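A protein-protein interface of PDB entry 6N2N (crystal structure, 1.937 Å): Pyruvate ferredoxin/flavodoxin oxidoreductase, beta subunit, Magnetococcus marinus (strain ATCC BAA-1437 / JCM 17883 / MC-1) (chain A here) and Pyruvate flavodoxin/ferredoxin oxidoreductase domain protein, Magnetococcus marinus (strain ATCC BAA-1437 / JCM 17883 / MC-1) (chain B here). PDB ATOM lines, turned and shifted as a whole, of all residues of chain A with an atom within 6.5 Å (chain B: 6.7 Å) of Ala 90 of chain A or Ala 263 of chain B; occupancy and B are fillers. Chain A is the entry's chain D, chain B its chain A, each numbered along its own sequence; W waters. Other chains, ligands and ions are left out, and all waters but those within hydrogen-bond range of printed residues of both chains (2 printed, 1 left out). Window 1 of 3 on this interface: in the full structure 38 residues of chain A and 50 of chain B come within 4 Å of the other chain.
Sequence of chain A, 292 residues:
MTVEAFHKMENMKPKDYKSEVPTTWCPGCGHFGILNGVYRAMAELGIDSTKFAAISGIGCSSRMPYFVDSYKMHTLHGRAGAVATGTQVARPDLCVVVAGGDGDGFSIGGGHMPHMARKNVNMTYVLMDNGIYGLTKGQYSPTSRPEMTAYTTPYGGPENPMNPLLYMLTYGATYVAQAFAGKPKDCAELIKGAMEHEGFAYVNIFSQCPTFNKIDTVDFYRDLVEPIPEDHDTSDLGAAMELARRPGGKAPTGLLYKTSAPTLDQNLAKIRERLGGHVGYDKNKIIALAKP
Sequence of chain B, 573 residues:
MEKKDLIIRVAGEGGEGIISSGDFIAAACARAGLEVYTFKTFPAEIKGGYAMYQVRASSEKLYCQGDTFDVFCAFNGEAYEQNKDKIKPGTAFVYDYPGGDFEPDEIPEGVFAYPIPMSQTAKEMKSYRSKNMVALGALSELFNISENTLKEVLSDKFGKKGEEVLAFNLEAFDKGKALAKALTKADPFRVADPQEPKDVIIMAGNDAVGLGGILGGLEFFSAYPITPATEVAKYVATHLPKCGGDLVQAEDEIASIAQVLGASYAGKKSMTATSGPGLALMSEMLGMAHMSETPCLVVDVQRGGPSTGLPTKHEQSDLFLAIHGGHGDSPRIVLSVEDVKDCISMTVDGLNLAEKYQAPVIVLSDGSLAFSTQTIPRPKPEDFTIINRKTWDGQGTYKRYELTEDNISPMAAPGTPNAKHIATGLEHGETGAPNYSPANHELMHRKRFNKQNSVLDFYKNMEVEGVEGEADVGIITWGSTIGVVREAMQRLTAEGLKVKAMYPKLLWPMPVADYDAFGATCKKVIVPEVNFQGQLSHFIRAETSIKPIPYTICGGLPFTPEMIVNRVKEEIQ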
ATOM      1  N   VAL A  83     -14.002 -23.700   1.927  1.00  0.00           N
ATOM      2  CA  VAL A  83     -13.678 -22.304   1.632  1.00  0.00           C
ATOM      3  C   VAL A  83     -12.828 -21.715   2.748  1.00  0.00           C
ATOM      4  O   VAL A  83     -11.814 -21.051   2.495  1.00  0.00           O
ATOM      5  CB  VAL A  83     -14.958 -21.474   1.413  1.00  0.00           C
ATOM      6  CG1 VAL A  83     -14.617 -19.982   1.382  1.00  0.00           C
ATOM      7  CG2 VAL A  83     -15.660 -21.888   0.130  1.00  0.00           C
ATOM      8  N   THR A  85     -10.804 -23.118   4.819  1.00  0.00           N
ATOM      9  CA  THR A  85      -9.430 -23.614   4.769  1.00  0.00           C
ATOM     10  C   THR A  85      -8.573 -22.726   3.874  1.00  0.00           C
ATOM     11  O   THR A  85      -7.455 -22.347   4.242  1.00  0.00           O
ATOM     12  CB  THR A  85      -9.404 -25.062   4.271  1.00  0.00           C
ATOM     13  OG1 THR A  85     -10.170 -25.897   5.147  1.00  0.00           O
ATOM     14  CG2 THR A  85      -7.967 -25.594   4.203  1.00  0.00           C
ATOM     15  N   GLY A  86      -9.095 -22.372   2.695  1.00  0.00           N
ATOM     16  CA  GLY A  86      -8.362 -21.485   1.808  1.00  0.00           C
ATOM     17  C   GLY A  86      -8.156 -20.108   2.406  1.00  0.00           C
ATOM     18  O   GLY A  86      -7.089 -19.511   2.263  1.00  0.00           O
ATOM     19  N   THR A  87      -9.184 -19.574   3.070  1.00  0.00           N
ATOM     20  CA  THR A  87      -9.041 -18.289   3.751  1.00  0.00           C
ATOM     21  C   THR A  87      -7.993 -18.374   4.855  1.00  0.00           C
ATOM     22  O   THR A  87      -7.121 -17.502   4.971  1.00  0.00           O
ATOM     23  CB  THR A  87     -10.391 -17.854   4.324  1.00  0.00           C
ATOM     24  OG1 THR A  87     -11.345 -17.749   3.261  1.00  0.00           O
ATOM     25  CG2 THR A  87     -10.268 -16.505   5.019  1.00  0.00           C
ATOM     26  N   GLN A  88      -8.050 -19.438   5.660  1.00  0.00           N
ATOM     27  CA  GLN A  88      -7.161 -19.573   6.809  1.00  0.00           C
ATOM     28  C   GLN A  88      -5.710 -19.734   6.370  1.00  0.00           C
ATOM     29  O   GLN A  88      -4.814 -19.054   6.887  1.00  0.00           O
ATOM     30  CB  GLN A  88      -7.606 -20.764   7.662  1.00  0.00           C
ATOM     31  CG  GLN A  88      -7.053 -20.787   9.084  1.00  0.00           C
ATOM     32  CD  GLN A  88      -5.614 -21.294   9.177  1.00  0.00           C
ATOM     33  OE1 GLN A  88      -5.218 -22.232   8.479  1.00  0.00           O
ATOM     34  NE2 GLN A  88      -4.835 -20.681  10.060  1.00  0.00           N
ATOM     35  N   VAL A  89      -5.462 -20.624   5.403  1.00  0.00           N
ATOM     36  CA  VAL A  89      -4.097 -20.854   4.935  1.00  0.00           C
ATOM     37  C   VAL A  89      -3.550 -19.596   4.269  1.00  0.00           C
ATOM     38  O   VAL A  89      -2.381 -19.240   4.447  1.00  0.00           O
ATOM     39  CB  VAL A  89      -4.055 -22.074   3.992  1.00  0.00           C
ATOM     40  CG1 VAL A  89      -2.752 -22.104   3.197  1.00  0.00           C
ATOM     41  CG2 VAL A  89      -4.232 -23.366   4.782  1.00  0.00           C
ATOM     42  N   ALA A  90      -4.398 -18.882   3.528  1.00  0.00           N
ATOM     43  CA  ALA A  90      -3.962 -17.644   2.891  1.00  0.00           C
ATOM     44  C   ALA A  90      -3.600 -16.576   3.921  1.00  0.00           C
ATOM     45  O   ALA A  90      -2.665 -15.796   3.709  1.00  0.00           O
ATOM     46  CB  ALA A  90      -5.057 -17.127   1.953  1.00  0.00           C
ATOM     47  N   ARG A  91      -4.324 -16.524   5.039  1.00  0.00           N
ATOM     48  CA  ARG A  91      -4.158 -15.465   6.041  1.00  0.00           C
ATOM     49  C   ARG A  91      -4.215 -16.073   7.432  1.00  0.00           C
ATOM     50  O   ARG A  91      -5.234 -15.980   8.126  1.00  0.00           O
ATOM     51  CB  ARG A  91      -5.228 -14.382   5.880  1.00  0.00           C
ATOM     52  CG  ARG A  91      -5.090 -13.539   4.619  1.00  0.00           C
ATOM     53  CD  ARG A  91      -3.935 -12.549   4.731  1.00  0.00           C
ATOM     54  NE  ARG A  91      -4.102 -11.693   5.901  1.00  0.00           N
ATOM     55  CZ  ARG A  91      -4.853 -10.598   5.918  1.00  0.00           C
ATOM     56  NH1 ARG A  91      -5.500 -10.219   4.821  1.00  0.00           N
ATOM     57  NH2 ARG A  91      -4.963  -9.886   7.033  1.00  0.00           N
ATOM     58  N   PRO A  92      -3.123 -16.702   7.882  1.00  0.00           N
ATOM     59  CA  PRO A  92      -3.130 -17.349   9.207  1.00  0.00           C
ATOM     60  C   PRO A  92      -3.259 -16.380  10.375  1.00  0.00           C
ATOM     61  O   PRO A  92      -3.398 -16.837  11.518  1.00  0.00           O
ATOM     62  CB  PRO A  92      -1.778 -18.083   9.250  1.00  0.00           C
ATOM     63  CG  PRO A  92      -1.354 -18.204   7.820  1.00  0.00           C
ATOM     64  CD  PRO A  92      -1.875 -16.966   7.147  1.00  0.00           C
ATOM     65  N   ASP A  93      -3.187 -15.073  10.134  1.00  0.00           N
ATOM     66  CA  ASP A  93      -3.407 -14.088  11.185  1.00  0.00           C
ATOM     67  C   ASP A  93      -4.876 -13.933  11.557  1.00  0.00           C
ATOM     68  O   ASP A  93      -5.172 -13.420  12.639  1.00  0.00           O
ATOM     69  CB  ASP A  93      -2.865 -12.729  10.750  1.00  0.00           C
ATOM     70  CG  ASP A  93      -3.428 -12.288   9.413  1.00  0.00           C
ATOM     71  OD1 ASP A  93      -3.323 -13.068   8.443  1.00  0.00           O
ATOM     72  OD2 ASP A  93      -3.999 -11.177   9.333  1.00  0.00           O
ATOM     73  N   PHE B 220      -1.442 -18.744  -3.891  1.00  0.00           N
ATOM     74  CA  PHE B 220      -2.102 -19.919  -3.339  1.00  0.00           C
ATOM     75  C   PHE B 220      -2.586 -20.828  -4.460  1.00  0.00           C
ATOM     76  O   PHE B 220      -3.297 -20.385  -5.365  1.00  0.00           O
ATOM     77  CB  PHE B 220      -3.286 -19.529  -2.434  1.00  0.00           C
ATOM     78  CG  PHE B 220      -4.034 -20.718  -1.894  1.00  0.00           C
ATOM     79  CD1 PHE B 220      -3.591 -21.374  -0.755  1.00  0.00           C
ATOM     80  CD2 PHE B 220      -5.156 -21.201  -2.543  1.00  0.00           C
ATOM     81  CE1 PHE B 220      -4.268 -22.479  -0.268  1.00  0.00           C
ATOM     82  CE2 PHE B 220      -5.827 -22.311  -2.067  1.00  0.00           C
ATOM     83  CZ  PHE B 220      -5.383 -22.946  -0.927  1.00  0.00           C
ATOM     84  N   PHE B 221      -2.229 -22.104  -4.371  1.00  0.00           N
ATOM     85  CA  PHE B 221      -2.607 -23.099  -5.366  1.00  0.00           C
ATOM     86  C   PHE B 221      -3.228 -24.284  -4.647  1.00  0.00           C
ATOM     87  O   PHE B 221      -2.666 -24.774  -3.665  1.00  0.00           O
ATOM     88  CB  PHE B 221      -1.380 -23.542  -6.171  1.00  0.00           C
ATOM     89  CG  PHE B 221      -1.696 -24.402  -7.367  1.00  0.00           C
ATOM     90  CD1 PHE B 221      -2.008 -25.739  -7.220  1.00  0.00           C
ATOM     91  CD2 PHE B 221      -1.642 -23.870  -8.646  1.00  0.00           C
ATOM     92  CE1 PHE B 221      -2.267 -26.530  -8.322  1.00  0.00           C
ATOM     93  CE2 PHE B 221      -1.905 -24.653  -9.753  1.00  0.00           C
ATOM     94  CZ  PHE B 221      -2.216 -25.987  -9.591  1.00  0.00           C
ATOM     95  N   ASP B 246       1.941 -20.960  -1.202  1.00  0.00           N
ATOM     96  CA  ASP B 246       1.573 -22.280  -0.703  1.00  0.00           C
ATOM     97  C   ASP B 246       0.777 -23.049  -1.744  1.00  0.00           C
ATOM     98  O   ASP B 246      -0.134 -22.503  -2.378  1.00  0.00           O
ATOM     99  CB  ASP B 246       0.737 -22.201   0.585  1.00  0.00           C
ATOM    100  CG  ASP B 246       1.511 -21.622   1.755  1.00  0.00           C
ATOM    101  OD1 ASP B 246       2.630 -22.101   2.031  1.00  0.00           O
ATOM    102  OD2 ASP B 246       1.000 -20.680   2.397  1.00  0.00           O
ATOM    103  N   ALA B 258     -13.080 -24.484  -3.982  1.00  0.00           N
ATOM    104  CA  ALA B 258     -13.560 -23.847  -2.761  1.00  0.00           C
ATOM    105  C   ALA B 258     -12.421 -23.150  -2.030  1.00  0.00           C
ATOM    106  O   ALA B 258     -12.546 -21.987  -1.625  1.00  0.00           O
ATOM    107  CB  ALA B 258     -14.227 -24.889  -1.862  1.00  0.00           C
ATOM    108  N   GLN B 259     -11.287 -23.842  -1.872  1.00  0.00           N
ATOM    109  CA  GLN B 259     -10.122 -23.246  -1.220  1.00  0.00           C
ATOM    110  C   GLN B 259      -9.583 -22.064  -2.020  1.00  0.00           C
ATOM    111  O   GLN B 259      -9.117 -21.076  -1.440  1.00  0.00           O
ATOM    112  CB  GLN B 259      -9.030 -24.305  -1.030  1.00  0.00           C
ATOM    113  CG  GLN B 259      -9.379 -25.407  -0.030  1.00  0.00           C
ATOM    114  CD  GLN B 259      -8.336 -26.521   0.001  1.00  0.00           C
ATOM    115  OE1 GLN B 259      -7.362 -26.496  -0.755  1.00  0.00           O
ATOM    116  NE2 GLN B 259      -8.533 -27.495   0.880  1.00  0.00           N
ATOM    117  N   VAL B 260      -9.620 -22.152  -3.354  1.00  0.00           N
ATOM    118  CA  VAL B 260      -9.208 -21.023  -4.190  1.00  0.00           C
ATOM    119  C   VAL B 260     -10.055 -19.792  -3.882  1.00  0.00           C
ATOM    120  O   VAL B 260      -9.529 -18.688  -3.693  1.00  0.00           O
ATOM    121  CB  VAL B 260      -9.291 -21.406  -5.679  1.00  0.00           C
ATOM    122  CG1 VAL B 260      -9.225 -20.174  -6.556  1.00  0.00           C
ATOM    123  CG2 VAL B 260      -8.162 -22.366  -6.036  1.00  0.00           C
ATOM    124  N   LEU B 261     -11.379 -19.965  -3.806  1.00  0.00           N
ATOM    125  CA  LEU B 261     -12.254 -18.825  -3.543  1.00  0.00           C
ATOM    126  C   LEU B 261     -12.018 -18.252  -2.153  1.00  0.00           C
ATOM    127  O   LEU B 261     -12.042 -17.029  -1.972  1.00  0.00           O
ATOM    128  CB  LEU B 261     -13.722 -19.222  -3.701  1.00  0.00           C
ATOM    129  CG  LEU B 261     -14.223 -19.446  -5.129  1.00  0.00           C
ATOM    130  CD1 LEU B 261     -15.717 -19.165  -5.193  1.00  0.00           C
ATOM    131  CD2 LEU B 261     -13.466 -18.573  -6.126  1.00  0.00           C
ATOM    132  N   GLY B 262     -11.790 -19.116  -1.164  1.00  0.00           N
ATOM    133  CA  GLY B 262     -11.517 -18.623   0.176  1.00  0.00           C
ATOM    134  C   GLY B 262     -10.201 -17.873   0.251  1.00  0.00           C
ATOM    135  O   GLY B 262     -10.110 -16.823   0.896  1.00  0.00           O
ATOM    136  N   ALA B 263      -9.169 -18.383  -0.433  1.00  0.00           N
ATOM    137  CA  ALA B 263      -7.886 -17.682  -0.458  1.00  0.00           C
ATOM    138  C   ALA B 263      -7.992 -16.375  -1.230  1.00  0.00           C
ATOM    139  O   ALA B 263      -7.381 -15.369  -0.851  1.00  0.00           O
ATOM    140  CB  ALA B 263      -6.809 -18.585  -1.062  1.00  0.00           C
ATOM    141  N   SER B 264      -8.787 -16.363  -2.303  1.00  0.00           N
ATOM    142  CA  SER B 264      -8.987 -15.137  -3.063  1.00  0.00           C
ATOM    143  C   SER B 264      -9.764 -14.102  -2.250  1.00  0.00           C
ATOM    144  O   SER B 264      -9.416 -12.915  -2.250  1.00  0.00           O
ATOM    145  CB  SER B 264      -9.709 -15.457  -4.369  1.00  0.00           C
ATOM    146  OG  SER B 264      -9.785 -14.319  -5.207  1.00  0.00           O
ATOM    147  N   TYR B 265     -10.815 -14.532  -1.550  1.00  0.00           N
ATOM    148  CA  TYR B 265     -11.509 -13.624  -0.637  1.00  0.00           C
ATOM    149  C   TYR B 265     -10.546 -13.031   0.387  1.00  0.00           C
ATOM    150  O   TYR B 265     -10.644 -11.846   0.735  1.00  0.00           O
ATOM    151  CB  TYR B 265     -12.635 -14.357   0.086  1.00  0.00           C
ATOM    152  CG  TYR B 265     -13.332 -13.487   1.115  1.00  0.00           C
ATOM    153  CD1 TYR B 265     -14.220 -12.502   0.719  1.00  0.00           C
ATOM    154  CD2 TYR B 265     -13.080 -13.632   2.471  1.00  0.00           C
ATOM    155  CE1 TYR B 265     -14.864 -11.696   1.643  1.00  0.00           C
ATOM    156  CE2 TYR B 265     -13.718 -12.822   3.408  1.00  0.00           C
ATOM    157  CZ  TYR B 265     -14.606 -11.861   2.985  1.00  0.00           C
ATOM    158  OH  TYR B 265     -15.242 -11.049   3.910  1.00  0.00           O
ATOM    159  N   ALA B 266      -9.612 -13.845   0.883  1.00  0.00           N
ATOM    160  CA  ALA B 266      -8.594 -13.386   1.821  1.00  0.00           C
ATOM    161  C   ALA B 266      -7.597 -12.419   1.188  1.00  0.00           C
ATOM    162  O   ALA B 266      -6.778 -11.842   1.913  1.00  0.00           O
ATOM    163  CB  ALA B 266      -7.858 -14.591   2.414  1.00  0.00           C
ATOM    164  N   GLY B 267      -7.657 -12.218  -0.128  1.00  0.00           N
ATOM    165  CA  GLY B 267      -6.839 -11.235  -0.807  1.00  0.00           C
ATOM    166  C   GLY B 267      -5.681 -11.779  -1.622  1.00  0.00           C
ATOM    167  O   GLY B 267      -4.880 -10.981  -2.128  1.00  0.00           O
ATOM    168  N   LYS B 268      -5.581 -13.096  -1.794  1.00  0.00           N
ATOM    169  CA  LYS B 268      -4.449 -13.726  -2.463  1.00  0.00           C
ATOM    170  C   LYS B 268      -4.805 -14.152  -3.885  1.00  0.00           C
ATOM    171  O   LYS B 268      -5.913 -14.628  -4.146  1.00  0.00           O
ATOM    172  CB  LYS B 268      -3.981 -14.948  -1.675  1.00  0.00           C
ATOM    173  CG  LYS B 268      -3.538 -14.655  -0.244  1.00  0.00           C
ATOM    174  CD  LYS B 268      -2.352 -13.713  -0.208  1.00  0.00           C
ATOM    175  CE  LYS B 268      -1.880 -13.486   1.226  1.00  0.00           C
ATOM    176  NZ  LYS B 268      -0.904 -12.363   1.317  1.00  0.00           N
ATOM    177  N   LYS B 269      -3.851 -13.991  -4.798  1.00  0.00           N
ATOM    178  CA  LYS B 269      -4.002 -14.509  -6.151  1.00  0.00           C
ATOM    179  C   LYS B 269      -3.947 -16.034  -6.115  1.00  0.00           C
ATOM    180  O   LYS B 269      -2.947 -16.610  -5.678  1.00  0.00           O
ATOM    181  CB  LYS B 269      -2.906 -13.949  -7.051  1.00  0.00           C
ATOM    182  CG  LYS B 269      -2.941 -12.441  -7.174  1.00  0.00           C
ATOM    183  CD  LYS B 269      -1.960 -11.930  -8.210  1.00  0.00           C
ATOM    184  CE  LYS B 269      -2.033 -10.411  -8.325  1.00  0.00           C
ATOM    185  NZ  LYS B 269      -1.093  -9.869  -9.342  1.00  0.00           N
ATOM    186  N   SER B 270      -5.019 -16.685  -6.564  1.00  0.00           N
ATOM    187  CA  SER B 270      -5.212 -18.117  -6.368  1.00  0.00           C
ATOM    188  C   SER B 270      -5.656 -18.770  -7.669  1.00  0.00           C
ATOM    189  O   SER B 270      -6.310 -18.140  -8.505  1.00  0.00           O
ATOM    190  CB  SER B 270      -6.266 -18.394  -5.264  1.00  0.00           C
ATOM    191  OG  SER B 270      -5.941 -17.721  -4.062  1.00  0.00           O
ATOM    192  N   THR B 294     -15.628 -12.740  -7.140  1.00  0.00           N
ATOM    193  CA  THR B 294     -14.385 -13.109  -6.482  1.00  0.00           C
ATOM    194  C   THR B 294     -13.410 -13.652  -7.515  1.00  0.00           C
ATOM    195  O   THR B 294     -13.737 -14.632  -8.202  1.00  0.00           O
ATOM    196  CB  THR B 294     -14.641 -14.149  -5.393  1.00  0.00           C
ATOM    197  OG1 THR B 294     -15.574 -13.620  -4.439  1.00  0.00           O
ATOM    198  CG2 THR B 294     -13.341 -14.481  -4.674  1.00  0.00           C
ATOM    199  N   ARG B 389      -5.977  -6.545  -8.293  1.00  0.00           N
ATOM    200  CA  ARG B 389      -7.376  -6.195  -8.093  1.00  0.00           C
ATOM    201  C   ARG B 389      -7.502  -4.751  -7.622  1.00  0.00           C
ATOM    202  O   ARG B 389      -6.689  -4.267  -6.830  1.00  0.00           O
ATOM    203  CB  ARG B 389      -8.006  -7.136  -7.064  1.00  0.00           C
ATOM    204  CG  ARG B 389      -7.291  -7.119  -5.715  1.00  0.00           C
ATOM    205  CD  ARG B 389      -7.761  -8.257  -4.839  1.00  0.00           C
ATOM    206  NE  ARG B 389      -7.443  -9.556  -5.434  1.00  0.00           N
ATOM    207  CZ  ARG B 389      -7.871 -10.720  -4.956  1.00  0.00           C
ATOM    208  NH1 ARG B 389      -8.651 -10.752  -3.879  1.00  0.00           N
ATOM    209  NH2 ARG B 389      -7.537 -11.851  -5.562  1.00  0.00           N
HETATM  210  O   HOH W   1      -9.769 -28.475   3.992  1.00  0.00           O
HETATM  211  O   HOH W   2      -4.419 -10.651   2.065  1.00  0.00           O
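The backbone carbonyl oxygen (O) of Gly 262 of chain B lies within hydrogen-bond range of the side-chain hydroxyl (OG1) of Thr 87 of chain A, 2.8 Å away.
The backbone NH (N) of Phe 220 of chain B sits at hydrogen-bond distance from the backbone carbonyl oxygen (O) of Lys 269 of chain B.
N of Lys 268 of chain B is in hydrogen-bond range of O of Ala 263 of chain B.
The side-chain hydroxyl (OG) of Ser 270 of chain B sits at hydrogen-bond distance from the backbone carbonyl oxygen (O) of Lys 268 of chain B (3.1 Å).
OG1 of Thr 87 of chain A lies within hydrogen-bond range of O of Val 83 of chain A (3.4 Å).
The side-chain carboxylate (OD2) of Asp 93 of chain A is in salt-bridge range of the guanidinium group (NH2) of Arg 91 of chain A (2.8 Å).
Val 83 of chain A touches Ala 258 of chain B.
Val 83 of chain A touches Gly 262 of chain B.
Gln 259 of chain B touches Gly 86 of chain A.
Gly 86 of chain A touches Gly 262 of chain B (C to C, 3.7 Å).
Ala 263 of chain B touches Gly 86 of chain A.
N of Ala 263 of chain B touches N of Thr 87 of chain A, at 3.7 Å.
Ala 266 of chain B touches Thr 87 of chain A.
CE1 of Phe 220 of chain B touches CG1 of Val 89 of chain A, at 3.8 Å.
Lys 268 of chain B touches Ala 90 of chain A (CE to O, 3.5 Å).
NH1 of Arg 91 of chain A touches O of Ala 266 of chain B, 3.6 Å away.
Printed residues of chain B within 4 Å of Thr 87 of chain A: Gly 262 (2.8 Å), Ala 263 (3.7 Å) and Ala 266 (3.9 Å).
Of chain B, only Ala 263 (3.8 Å), Ala 266 (3.8 Å) and Lys 268 (3.5 Å) come within 4 Å of Ala 90 of chain A.
Printed residues of chain B within 4 Å of Arg 91 of chain A: Ala 266.
Printed residues of chain A within 4 Å of Ala 258 of chain B: Val 83.
Of chain A, only Gly 86 (3.4 Å), Thr 87 (3.7 Å) and Ala 90 (3.8 Å) come within 4 Å of Ala 263 of chain B.
Tyr 265 of chain B touches none of the printed residues of chain A.
Lys 269 of chain B touches none of the printed residues of chain A.
Of the 18 printed residues of chain B, 7 touch a printed residue of chain A.
Printed residues of chain B that touch a printed residue of chain A: Phe 220, Ala 258, Gln 259, Gly 262, Ala 263, Ala 266 and Lys 268.
Along chain A the printed residues that touch a printed residue of chain B span positions 83 to 91.
Among the printed residues, 14 pairs touch across the chains.
Among the printed residues, no Asp or Glu carboxylate lies within 4 Å of a Lys or Arg side-chain nitrogen of the other chain.
Water W2 lies within hydrogen-bond range of the backbone carbonyl oxygen (O) of Ala 266 of chain B (2.6 Å) and the guanidinium group (NH1) of Arg 91 of chain A (3.0 Å).
Water W1 lies within hydrogen-bond range of OG1 of Thr 85 of chain A and NE2 of Gln 259 of chain B.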
